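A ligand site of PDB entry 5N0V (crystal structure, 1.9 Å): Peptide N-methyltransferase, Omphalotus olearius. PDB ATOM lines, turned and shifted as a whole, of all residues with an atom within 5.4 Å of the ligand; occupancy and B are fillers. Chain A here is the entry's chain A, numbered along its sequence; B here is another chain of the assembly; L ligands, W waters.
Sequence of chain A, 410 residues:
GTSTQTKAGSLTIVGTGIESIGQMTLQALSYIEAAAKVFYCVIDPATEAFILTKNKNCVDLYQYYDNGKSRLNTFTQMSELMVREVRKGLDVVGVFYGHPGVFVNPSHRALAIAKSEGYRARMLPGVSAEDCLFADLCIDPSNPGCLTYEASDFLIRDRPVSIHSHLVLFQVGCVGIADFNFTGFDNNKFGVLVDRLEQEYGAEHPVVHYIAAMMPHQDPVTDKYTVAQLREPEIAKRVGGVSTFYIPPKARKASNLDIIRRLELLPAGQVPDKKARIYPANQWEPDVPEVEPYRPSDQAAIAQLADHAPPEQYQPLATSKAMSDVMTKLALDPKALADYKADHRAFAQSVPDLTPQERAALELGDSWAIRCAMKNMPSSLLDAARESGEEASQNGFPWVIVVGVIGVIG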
ATOM      1  N   ILE A  18      26.369  -2.397 -35.474  1.00  0.00           N
ATOM      2  CA  ILE A  18      25.413  -3.155 -34.641  1.00  0.00           C
ATOM      3  C   ILE A  18      24.165  -3.528 -35.415  1.00  0.00           C
ATOM      4  O   ILE A  18      23.741  -4.694 -35.388  1.00  0.00           O
ATOM      5  CB  ILE A  18      25.044  -2.354 -33.376  1.00  0.00           C
ATOM      6  CG1 ILE A  18      26.299  -2.095 -32.543  1.00  0.00           C
ATOM      7  CG2 ILE A  18      23.948  -3.056 -32.573  1.00  0.00           C
ATOM      8  CD1 ILE A  18      26.979  -3.319 -31.959  1.00  0.00           C
ATOM      9  N   ILE A  43      26.279 -11.347 -35.398  1.00  0.00           N
ATOM     10  CA  ILE A  43      25.152 -11.837 -34.572  1.00  0.00           C
ATOM     11  C   ILE A  43      23.886 -12.173 -35.359  1.00  0.00           C
ATOM     12  O   ILE A  43      23.110 -13.011 -34.894  1.00  0.00           O
ATOM     13  CB  ILE A  43      24.774 -10.896 -33.401  1.00  0.00           C
ATOM     14  CG1 ILE A  43      25.968 -10.754 -32.452  1.00  0.00           C
ATOM     15  CG2 ILE A  43      23.568 -11.447 -32.630  1.00  0.00           C
ATOM     16  CD1 ILE A  43      25.669 -10.067 -31.131  1.00  0.00           C
ATOM     17  N   TYR A  97      31.287  -8.033 -35.220  1.00  0.00           N
ATOM     18  CA  TYR A  97      30.123  -7.235 -34.807  1.00  0.00           C
ATOM     19  C   TYR A  97      30.545  -5.892 -34.189  1.00  0.00           C
ATOM     20  O   TYR A  97      31.518  -5.842 -33.436  1.00  0.00           O
ATOM     21  CB  TYR A  97      29.359  -8.069 -33.775  1.00  0.00           C
ATOM     22  CG  TYR A  97      28.082  -7.511 -33.184  1.00  0.00           C
ATOM     23  CD1 TYR A  97      26.988  -7.155 -33.968  1.00  0.00           C
ATOM     24  CD2 TYR A  97      27.930  -7.456 -31.801  1.00  0.00           C
ATOM     25  CE1 TYR A  97      25.801  -6.698 -33.400  1.00  0.00           C
ATOM     26  CE2 TYR A  97      26.759  -7.004 -31.215  1.00  0.00           C
ATOM     27  CZ  TYR A  97      25.693  -6.624 -31.999  1.00  0.00           C
ATOM     28  OH  TYR A  97      24.545  -6.194 -31.373  1.00  0.00           O
ATOM     29  N   GLY A  98      29.845  -4.815 -34.547  1.00  0.00           N
ATOM     30  CA  GLY A  98      30.101  -3.511 -33.949  1.00  0.00           C
ATOM     31  C   GLY A  98      31.413  -2.916 -34.428  1.00  0.00           C
ATOM     32  O   GLY A  98      31.693  -2.906 -35.632  1.00  0.00           O
ATOM     33  N   HIS A  99      32.186  -2.402 -33.480  1.00  0.00           N
ATOM     34  CA  HIS A  99      33.567  -1.962 -33.669  1.00  0.00           C
ATOM     35  C   HIS A  99      34.443  -3.172 -33.296  1.00  0.00           C
ATOM     36  O   HIS A  99      34.311  -3.723 -32.201  1.00  0.00           O
ATOM     37  CB  HIS A  99      33.837  -0.774 -32.732  1.00  0.00           C
ATOM     38  CG  HIS A  99      35.200  -0.154 -32.854  1.00  0.00           C
ATOM     39  ND1 HIS A  99      36.365  -0.891 -32.883  1.00  0.00           N
ATOM     40  CD2 HIS A  99      35.577   1.149 -32.873  1.00  0.00           C
ATOM     41  CE1 HIS A  99      37.404  -0.060 -32.948  1.00  0.00           C
ATOM     42  NE2 HIS A  99      36.947   1.175 -32.939  1.00  0.00           N
ATOM     43  N   PRO A 100      35.339  -3.607 -34.198  1.00  0.00           N
ATOM     44  CA  PRO A 100      36.059  -4.874 -33.990  1.00  0.00           C
ATOM     45  C   PRO A 100      37.115  -4.886 -32.881  1.00  0.00           C
ATOM     46  O   PRO A 100      37.703  -5.945 -32.637  1.00  0.00           O
ATOM     47  CB  PRO A 100      36.750  -5.092 -35.328  1.00  0.00           C
ATOM     48  CG  PRO A 100      37.001  -3.720 -35.840  1.00  0.00           C
ATOM     49  CD  PRO A 100      35.762  -2.938 -35.449  1.00  0.00           C
ATOM     50  N   VAL A 102      36.312  -3.060 -29.814  1.00  0.00           N
ATOM     51  CA  VAL A 102      35.573  -2.593 -28.631  1.00  0.00           C
ATOM     52  C   VAL A 102      34.968  -3.817 -27.963  1.00  0.00           C
ATOM     53  O   VAL A 102      34.034  -4.415 -28.499  1.00  0.00           O
ATOM     54  CB  VAL A 102      34.513  -1.539 -29.030  1.00  0.00           C
ATOM     55  CG1 VAL A 102      33.544  -1.216 -27.887  1.00  0.00           C
ATOM     56  CG2 VAL A 102      35.194  -0.264 -29.485  1.00  0.00           C
ATOM     57  N   PHE A 103      35.502  -4.181 -26.796  1.00  0.00           N
ATOM     58  CA  PHE A 103      35.120  -5.407 -26.104  1.00  0.00           C
ATOM     59  C   PHE A 103      35.284  -6.647 -27.033  1.00  0.00           C
ATOM     60  O   PHE A 103      34.361  -7.455 -27.163  1.00  0.00           O
ATOM     61  CB  PHE A 103      33.692  -5.282 -25.511  1.00  0.00           C
ATOM     62  CG  PHE A 103      33.554  -4.224 -24.443  1.00  0.00           C
ATOM     63  CD1 PHE A 103      33.643  -2.864 -24.772  1.00  0.00           C
ATOM     64  CD2 PHE A 103      33.336  -4.565 -23.115  1.00  0.00           C
ATOM     65  CE1 PHE A 103      33.526  -1.886 -23.789  1.00  0.00           C
ATOM     66  CE2 PHE A 103      33.225  -3.577 -22.145  1.00  0.00           C
ATOM     67  CZ  PHE A 103      33.315  -2.238 -22.481  1.00  0.00           C
ATOM     68  N   VAL A 104      36.456  -6.766 -27.653  1.00  0.00           N
ATOM     69  CA  VAL A 104      36.799  -7.918 -28.522  1.00  0.00           C
ATOM     70  C   VAL A 104      38.209  -8.425 -28.187  1.00  0.00           C
ATOM     71  O   VAL A 104      39.150  -7.645 -28.211  1.00  0.00           O
ATOM     72  CB  VAL A 104      36.752  -7.541 -30.027  1.00  0.00           C
ATOM     73  CG1 VAL A 104      36.954  -8.780 -30.923  1.00  0.00           C
ATOM     74  CG2 VAL A 104      35.429  -6.870 -30.388  1.00  0.00           C
ATOM     75  N   VAL A 127      31.078   1.103 -35.925  1.00  0.00           N
ATOM     76  CA  VAL A 127      30.088   1.647 -35.011  1.00  0.00           C
ATOM     77  C   VAL A 127      29.884   0.649 -33.887  1.00  0.00           C
ATOM     78  O   VAL A 127      29.485  -0.488 -34.129  1.00  0.00           O
ATOM     79  CB  VAL A 127      28.758   1.910 -35.748  1.00  0.00           C
ATOM     80  CG1 VAL A 127      27.621   2.184 -34.767  1.00  0.00           C
ATOM     81  CG2 VAL A 127      28.934   3.066 -36.726  1.00  0.00           C
ATOM     82  N   SER A 128      30.149   1.069 -32.646  1.00  0.00           N
ATOM     83  CA  SER A 128      29.970   0.224 -31.471  1.00  0.00           C
ATOM     84  C   SER A 128      28.580   0.339 -30.854  1.00  0.00           C
ATOM     85  O   SER A 128      27.794   1.231 -31.193  1.00  0.00           O
ATOM     86  CB  SER A 128      31.012   0.572 -30.398  1.00  0.00           C
ATOM     87  OG  SER A 128      30.706   1.801 -29.768  1.00  0.00           O
ATOM     88  N   ALA A 129      28.291  -0.563 -29.904  1.00  0.00           N
ATOM     89  CA  ALA A 129      27.081  -0.495 -29.080  1.00  0.00           C
ATOM     90  C   ALA A 129      26.963   0.823 -28.309  1.00  0.00           C
ATOM     91  O   ALA A 129      25.844   1.306 -28.093  1.00  0.00           O
ATOM     92  CB  ALA A 129      27.043  -1.657 -28.091  1.00  0.00           C
ATOM     93  N   GLU A 130      28.101   1.376 -27.893  1.00  0.00           N
ATOM     94  CA  GLU A 130      28.147   2.660 -27.193  1.00  0.00           C
ATOM     95  C   GLU A 130      27.843   3.825 -28.140  1.00  0.00           C
ATOM     96  O   GLU A 130      27.130   4.751 -27.764  1.00  0.00           O
ATOM     97  CB  GLU A 130      29.491   2.875 -26.486  1.00  0.00           C
ATOM     98  CG  GLU A 130      29.544   4.198 -25.733  1.00  0.00           C
ATOM     99  CD  GLU A 130      30.722   4.306 -24.785  1.00  0.00           C
ATOM    100  OE1 GLU A 130      31.811   4.764 -25.183  1.00  0.00           O
ATOM    101  OE2 GLU A 130      30.543   3.963 -23.600  1.00  0.00           O
ATOM    102  N   LEU A 169      27.888   0.589 -18.848  1.00  0.00           N
ATOM    103  CA  LEU A 169      28.340  -0.747 -18.455  1.00  0.00           C
ATOM    104  C   LEU A 169      27.930  -1.777 -19.501  1.00  0.00           C
ATOM    105  O   LEU A 169      26.753  -2.006 -19.735  1.00  0.00           O
ATOM    106  CB  LEU A 169      27.749  -1.123 -17.102  1.00  0.00           C
ATOM    107  CG  LEU A 169      28.126  -0.234 -15.922  1.00  0.00           C
ATOM    108  CD1 LEU A 169      27.352  -0.652 -14.667  1.00  0.00           C
ATOM    109  CD2 LEU A 169      29.623  -0.268 -15.663  1.00  0.00           C
ATOM    110  N   PHE A 170      28.930  -2.402 -20.114  1.00  0.00           N
ATOM    111  CA  PHE A 170      28.737  -3.487 -21.064  1.00  0.00           C
ATOM    112  C   PHE A 170      28.645  -4.821 -20.303  1.00  0.00           C
ATOM    113  O   PHE A 170      29.212  -4.957 -19.223  1.00  0.00           O
ATOM    114  CB  PHE A 170      29.933  -3.595 -22.013  1.00  0.00           C
ATOM    115  CG  PHE A 170      29.925  -2.624 -23.168  1.00  0.00           C
ATOM    116  CD1 PHE A 170      29.973  -1.242 -22.962  1.00  0.00           C
ATOM    117  CD2 PHE A 170      29.957  -3.088 -24.488  1.00  0.00           C
ATOM    118  CE1 PHE A 170      30.006  -0.357 -24.040  1.00  0.00           C
ATOM    119  CE2 PHE A 170      30.001  -2.212 -25.566  1.00  0.00           C
ATOM    120  CZ  PHE A 170      30.012  -0.844 -25.350  1.00  0.00           C
ATOM    121  N   GLN A 171      27.991  -5.803 -20.920  1.00  0.00           N
ATOM    122  CA  GLN A 171      27.957  -7.193 -20.422  1.00  0.00           C
ATOM    123  C   GLN A 171      27.310  -7.330 -19.044  1.00  0.00           C
ATOM    124  O   GLN A 171      27.727  -8.135 -18.213  1.00  0.00           O
ATOM    125  CB  GLN A 171      29.352  -7.819 -20.426  1.00  0.00           C
ATOM    126  CG  GLN A 171      30.157  -7.455 -21.669  1.00  0.00           C
ATOM    127  CD  GLN A 171      31.195  -8.493 -22.045  1.00  0.00           C
ATOM    128  OE1 GLN A 171      31.409  -8.736 -23.224  1.00  0.00           O
ATOM    129  NE2 GLN A 171      31.843  -9.096 -21.050  1.00  0.00           N
ATOM    130  N   VAL A 172      26.257  -6.539 -18.821  1.00  0.00           N
ATOM    131  CA  VAL A 172      25.494  -6.601 -17.585  1.00  0.00           C
ATOM    132  C   VAL A 172      24.682  -7.895 -17.431  1.00  0.00           C
ATOM    133  O   VAL A 172      24.250  -8.207 -16.330  1.00  0.00           O
ATOM    134  CB  VAL A 172      24.569  -5.379 -17.420  1.00  0.00           C
ATOM    135  CG1 VAL A 172      25.393  -4.122 -17.249  1.00  0.00           C
ATOM    136  CG2 VAL A 172      23.585  -5.241 -18.596  1.00  0.00           C
ATOM    137  N   TYR A 210      19.444  -0.651 -22.000  1.00  0.00           N
ATOM    138  CA  TYR A 210      19.562  -0.315 -23.398  1.00  0.00           C
ATOM    139  C   TYR A 210      19.872  -1.534 -24.270  1.00  0.00           C
ATOM    140  O   TYR A 210      20.813  -2.286 -23.988  1.00  0.00           O
ATOM    141  CB  TYR A 210      20.649   0.748 -23.616  1.00  0.00           C
ATOM    142  CG  TYR A 210      20.858   1.070 -25.074  1.00  0.00           C
ATOM    143  CD1 TYR A 210      19.838   1.636 -25.826  1.00  0.00           C
ATOM    144  CD2 TYR A 210      22.052   0.759 -25.709  1.00  0.00           C
ATOM    145  CE1 TYR A 210      20.007   1.903 -27.183  1.00  0.00           C
ATOM    146  CE2 TYR A 210      22.222   1.028 -27.056  1.00  0.00           C
ATOM    147  CZ  TYR A 210      21.195   1.605 -27.788  1.00  0.00           C
ATOM    148  OH  TYR A 210      21.370   1.877 -29.116  1.00  0.00           O
ATOM    149  N   ILE A 211      19.050  -1.728 -25.292  1.00  0.00           N
ATOM    150  CA  ILE A 211      19.356  -2.669 -26.374  1.00  0.00           C
ATOM    151  C   ILE A 211      19.137  -1.951 -27.721  1.00  0.00           C
ATOM    152  O   ILE A 211      18.005  -1.583 -28.053  1.00  0.00           O
ATOM    153  CB  ILE A 211      18.503  -3.954 -26.337  1.00  0.00           C
ATOM    154  CG1 ILE A 211      18.579  -4.596 -24.940  1.00  0.00           C
ATOM    155  CG2 ILE A 211      18.985  -4.935 -27.399  1.00  0.00           C
ATOM    156  CD1 ILE A 211      17.759  -5.862 -24.799  1.00  0.00           C
ATOM    157  N   ALA A 212      20.218  -1.754 -28.468  1.00  0.00           N
ATOM    158  CA  ALA A 212      20.144  -1.219 -29.826  1.00  0.00           C
ATOM    159  C   ALA A 212      19.390  -2.193 -30.723  1.00  0.00           C
ATOM    160  O   ALA A 212      19.566  -3.415 -30.600  1.00  0.00           O
ATOM    161  CB  ALA A 212      21.535  -0.990 -30.387  1.00  0.00           C
ATOM    162  N   ALA A 213      18.542  -1.667 -31.600  1.00  0.00           N
ATOM    163  CA  ALA A 213      17.928  -2.447 -32.673  1.00  0.00           C
ATOM    164  C   ALA A 213      19.027  -3.143 -33.473  1.00  0.00           C
ATOM    165  O   ALA A 213      19.983  -2.494 -33.894  1.00  0.00           O
ATOM    166  CB  ALA A 213      17.106  -1.544 -33.587  1.00  0.00           C
ATOM    167  N   MET A 214      18.901  -4.454 -33.663  1.00  0.00           N
ATOM    168  CA  MET A 214      19.840  -5.202 -34.511  1.00  0.00           C
ATOM    169  C   MET A 214      19.283  -5.434 -35.917  1.00  0.00           C
ATOM    170  O   MET A 214      20.047  -5.689 -36.840  1.00  0.00           O
ATOM    171  CB  MET A 214      20.264  -6.493 -33.819  1.00  0.00           C
ATOM    172  CG  MET A 214      21.240  -6.207 -32.670  1.00  0.00           C
ATOM    173  SD  MET A 214      21.109  -7.352 -31.279  1.00  0.00           S
ATOM    174  CE  MET A 214      21.981  -8.728 -32.009  1.00  0.00           C
ATOM    175  N   GLY A 240      19.873  -9.457 -20.765  1.00  0.00           N
ATOM    176  CA  GLY A 240      20.545 -10.590 -21.418  1.00  0.00           C
ATOM    177  C   GLY A 240      21.886 -10.232 -22.031  1.00  0.00           C
ATOM    178  O   GLY A 240      22.492  -9.211 -21.680  1.00  0.00           O
ATOM    179  N   GLY A 241      22.321 -11.081 -22.960  1.00  0.00           N
ATOM    180  CA  GLY A 241      23.657 -10.987 -23.558  1.00  0.00           C
ATOM    181  C   GLY A 241      23.948  -9.766 -24.416  1.00  0.00           C
ATOM    182  O   GLY A 241      25.122  -9.420 -24.606  1.00  0.00           O
ATOM    183  N   VAL A 242      22.911  -9.111 -24.930  1.00  0.00           N
ATOM    184  CA  VAL A 242      23.066  -7.859 -25.691  1.00  0.00           C
ATOM    185  C   VAL A 242      22.660  -6.604 -24.898  1.00  0.00           C
ATOM    186  O   VAL A 242      22.550  -5.522 -25.469  1.00  0.00           O
ATOM    187  CB  VAL A 242      22.341  -7.919 -27.057  1.00  0.00           C
ATOM    188  CG1 VAL A 242      22.952  -8.998 -27.935  1.00  0.00           C
ATOM    189  CG2 VAL A 242      20.842  -8.170 -26.915  1.00  0.00           C
ATOM    190  N   SER A 243      22.444  -6.742 -23.583  1.00  0.00           N
ATOM    191  CA  SER A 243      22.019  -5.610 -22.766  1.00  0.00           C
ATOM    192  C   SER A 243      23.215  -4.760 -22.339  1.00  0.00           C
ATOM    193  O   SER A 243      24.285  -5.292 -22.008  1.00  0.00           O
ATOM    194  CB  SER A 243      21.250  -6.090 -21.522  1.00  0.00           C
ATOM    195  OG  SER A 243      20.048  -6.768 -21.882  1.00  0.00           O
ATOM    196  N   THR A 244      23.033  -3.443 -22.352  1.00  0.00           N
ATOM    197  CA  THR A 244      24.011  -2.494 -21.832  1.00  0.00           C
ATOM    198  C   THR A 244      23.254  -1.569 -20.866  1.00  0.00           C
ATOM    199  O   THR A 244      22.080  -1.267 -21.105  1.00  0.00           O
ATOM    200  CB  THR A 244      24.657  -1.695 -22.988  1.00  0.00           C
ATOM    201  OG1 THR A 244      25.377  -2.600 -23.836  1.00  0.00           O
ATOM    202  CG2 THR A 244      25.642  -0.626 -22.500  1.00  0.00           C
ATOM    203  N   TRP B 399      29.042 -12.686 -27.027  1.00  0.00           N
ATOM    204  CA  TRP B 399      29.816 -11.637 -26.354  1.00  0.00           C
ATOM    205  C   TRP B 399      31.256 -12.149 -26.325  1.00  0.00           C
ATOM    206  O   TRP B 399      31.518 -13.308 -25.983  1.00  0.00           O
ATOM    207  CB  TRP B 399      29.277 -11.236 -24.975  1.00  0.00           C
ATOM    208  CG  TRP B 399      29.087 -12.341 -23.983  1.00  0.00           C
ATOM    209  CD1 TRP B 399      27.904 -12.980 -23.680  1.00  0.00           C
ATOM    210  CD2 TRP B 399      30.086 -12.920 -23.151  1.00  0.00           C
ATOM    211  NE1 TRP B 399      28.124 -13.930 -22.709  1.00  0.00           N
ATOM    212  CE2 TRP B 399      29.449 -13.920 -22.368  1.00  0.00           C
ATOM    213  CE3 TRP B 399      31.458 -12.709 -22.979  1.00  0.00           C
ATOM    214  CZ2 TRP B 399      30.147 -14.696 -21.428  1.00  0.00           C
ATOM    215  CZ3 TRP B 399      32.152 -13.488 -22.057  1.00  0.00           C
ATOM    216  CH2 TRP B 399      31.487 -14.464 -21.293  1.00  0.00           C
ATOM    217  N   VAL B 400      32.174 -11.282 -26.743  1.00  0.00           N
ATOM    218  CA  VAL B 400      33.437 -11.703 -27.364  1.00  0.00           C
ATOM    219  C   VAL B 400      34.688 -11.182 -26.626  1.00  0.00           C
ATOM    220  O   VAL B 400      35.763 -11.068 -27.222  1.00  0.00           O
ATOM    221  CB  VAL B 400      33.398 -11.347 -28.888  1.00  0.00           C
ATOM    222  CG1 VAL B 400      33.357  -9.842 -29.119  1.00  0.00           C
ATOM    223  CG2 VAL B 400      34.514 -12.009 -29.686  1.00  0.00           C
ATOM    224  N   ILE B 401      34.526 -10.862 -25.316  1.00  0.00           N
ATOM    225  CA  ILE B 401      35.663 -10.652 -24.397  1.00  0.00           C
ATOM    226  C   ILE B 401      35.513 -11.293 -23.033  1.00  0.00           C
ATOM    227  O   ILE B 401      34.431 -11.319 -22.460  1.00  0.00           O
ATOM    228  CB  ILE B 401      35.998  -9.182 -24.030  1.00  0.00           C
ATOM    229  CG1 ILE B 401      34.737  -8.383 -23.721  1.00  0.00           C
ATOM    230  CG2 ILE B 401      36.887  -8.512 -25.062  1.00  0.00           C
ATOM    231  CD1 ILE B 401      34.902  -7.493 -22.515  1.00  0.00           C
HETATM  232  N1  LIG L   1      32.303  -5.203 -30.302  1.00  0.00           N
HETATM  233  C1  LIG L   1      30.938  -4.943 -29.849  1.00  0.00           C
HETATM  234  C2  LIG L   1      30.724  -5.388 -28.390  1.00  0.00           C
HETATM  235  C3  LIG L   1      31.101  -6.833 -28.108  1.00  0.00           C
HETATM  236  S1  LIG L   1      30.897  -7.295 -26.400  1.00  0.00           S
HETATM  237  C4  LIG L   1      30.618  -3.478 -29.971  1.00  0.00           C
HETATM  238  O1  LIG L   1      31.252  -2.709 -30.715  1.00  0.00           O
HETATM  239  O2  LIG L   1      29.708  -2.975 -29.305  1.00  0.00           O
HETATM  240  C5  LIG L   1      29.159  -7.592 -26.240  1.00  0.00           C
HETATM  241  C6  LIG L   1      28.531  -6.513 -25.348  1.00  0.00           C
HETATM  242  O3  LIG L   1      28.320  -5.329 -26.111  1.00  0.00           O
HETATM  243  C7  LIG L   1      27.169  -6.848 -24.766  1.00  0.00           C
HETATM  244  O4  LIG L   1      27.258  -7.548 -23.518  1.00  0.00           O
HETATM  245  C8  LIG L   1      26.549  -5.473 -24.589  1.00  0.00           C
HETATM  246  O5  LIG L   1      26.966  -4.839 -23.376  1.00  0.00           O
HETATM  247  C9  LIG L   1      27.085  -4.708 -25.788  1.00  0.00           C
HETATM  248  N2  LIG L   1      26.098  -4.876 -26.882  1.00  0.00           N
HETATM  249  C10 LIG L   1      26.169  -5.735 -27.906  1.00  0.00           C
HETATM  250  N3  LIG L   1      25.073  -5.626 -28.700  1.00  0.00           N
HETATM  251  C11 LIG L   1      24.284  -4.691 -28.164  1.00  0.00           C
HETATM  252  C12 LIG L   1      22.987  -4.094 -28.498  1.00  0.00           C
HETATM  253  N4  LIG L   1      22.319  -4.509 -29.600  1.00  0.00           N
HETATM  254  N5  LIG L   1      22.501  -3.135 -27.680  1.00  0.00           N
HETATM  255  C13 LIG L   1      23.188  -2.718 -26.583  1.00  0.00           C
HETATM  256  N6  LIG L   1      24.376  -3.237 -26.228  1.00  0.00           N
HETATM  257  C14 LIG L   1      24.962  -4.192 -26.975  1.00  0.00           C
HETATM  258  O   HOH W   1      24.889  -7.888 -21.439  1.00  0.00           O
HETATM  259  O   HOH W   2      32.112  -7.755 -31.464  1.00  0.00           O
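N of Gln 171 sits at hydrogen-bond distance from O5 of the ligand, at 2.8 Å. SD of Met 214 is in hydrogen-bond range of N4 of the ligand (3.5 Å). The backbone carbonyl oxygen of His 99 lies within hydrogen-bond range of a nitrogen (N1) of the ligand (3.1 Å). The backbone carbonyl oxygen (O) of Gly 241 is in hydrogen-bond range of an oxygen (O4) of the ligand, 3.0 Å away. OE1 of Gln 171 sits close to S1 of the ligand (3.5 Å). N of His 99 is in hydrogen-bond range of O1 of the ligand, 2.9 Å away. O2 of the ligand lies within hydrogen-bond range of N of Ala 129 (2.9 Å). The backbone carbonyl oxygen of Tyr 97 is in hydrogen-bond range of a nitrogen (N1) of the ligand, at 3.3 Å. The backbone carbonyl oxygen (O) of Ala 212 is in hydrogen-bond range of a nitrogen (N4) of the ligand, at 3.1 Å. A nitrogen (N6) of the ligand sits at hydrogen-bond distance from the side-chain hydroxyl (OG1) of Thr 244 (2.7 Å). O of Ser 243 sits at hydrogen-bond distance from O5 of the ligand (3.0 Å). The backbone carbonyl oxygen (O) of Val 102 sits at hydrogen-bond distance from a nitrogen (N1) of the ligand, 2.6 Å away. OH of Tyr 97 lies within hydrogen-bond range of N3 of the ligand (2.8 Å). N5 of the ligand lies within hydrogen-bond range of N of Ala 212, at 2.8 Å.
O of Val 127 is in hydrogen-bond range of N of His 99 (3.4 Å). The backbone carbonyl oxygen of Thr 244 lies within hydrogen-bond range of the backbone NH of Tyr 210 (2.9 Å). OG of Ser 243 sits at hydrogen-bond distance from N of Gly 240, at 2.9 Å. OG of Ser 128 sits close to N of Glu 130 (3.2 Å). The side-chain hydroxyl (OH) of Tyr 97 sits close to the side-chain sulfur (SD) of Met 214 (3.6 Å).
S1 of the ligand sits close to O of Phe 103, 3.6 Å away. N6 of the ligand lies close to O of Val 242 (3.0 Å). Merely in contact with the ligand: Ile 18, Gly 98, Val 104, Ser 128, Phe 170, Tyr 210, Ile 211, Trp 399 of chain B and Val 400 of chain B. The nearest printed residue that does not touch the ligand is Val 127 (4.4 Å).
Water W2 bridges a nitrogen (N1) of the ligand (2.8 Å) and the backbone carbonyl oxygen (O) of Tyr 97 (2.8 Å). Water W1 lies within hydrogen-bond range of O of Ser 243 (2.7 Å), O of Gly 240 (2.7 Å), O4 of the ligand (3.2 Å) and N of Val 172 (3.2 Å).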
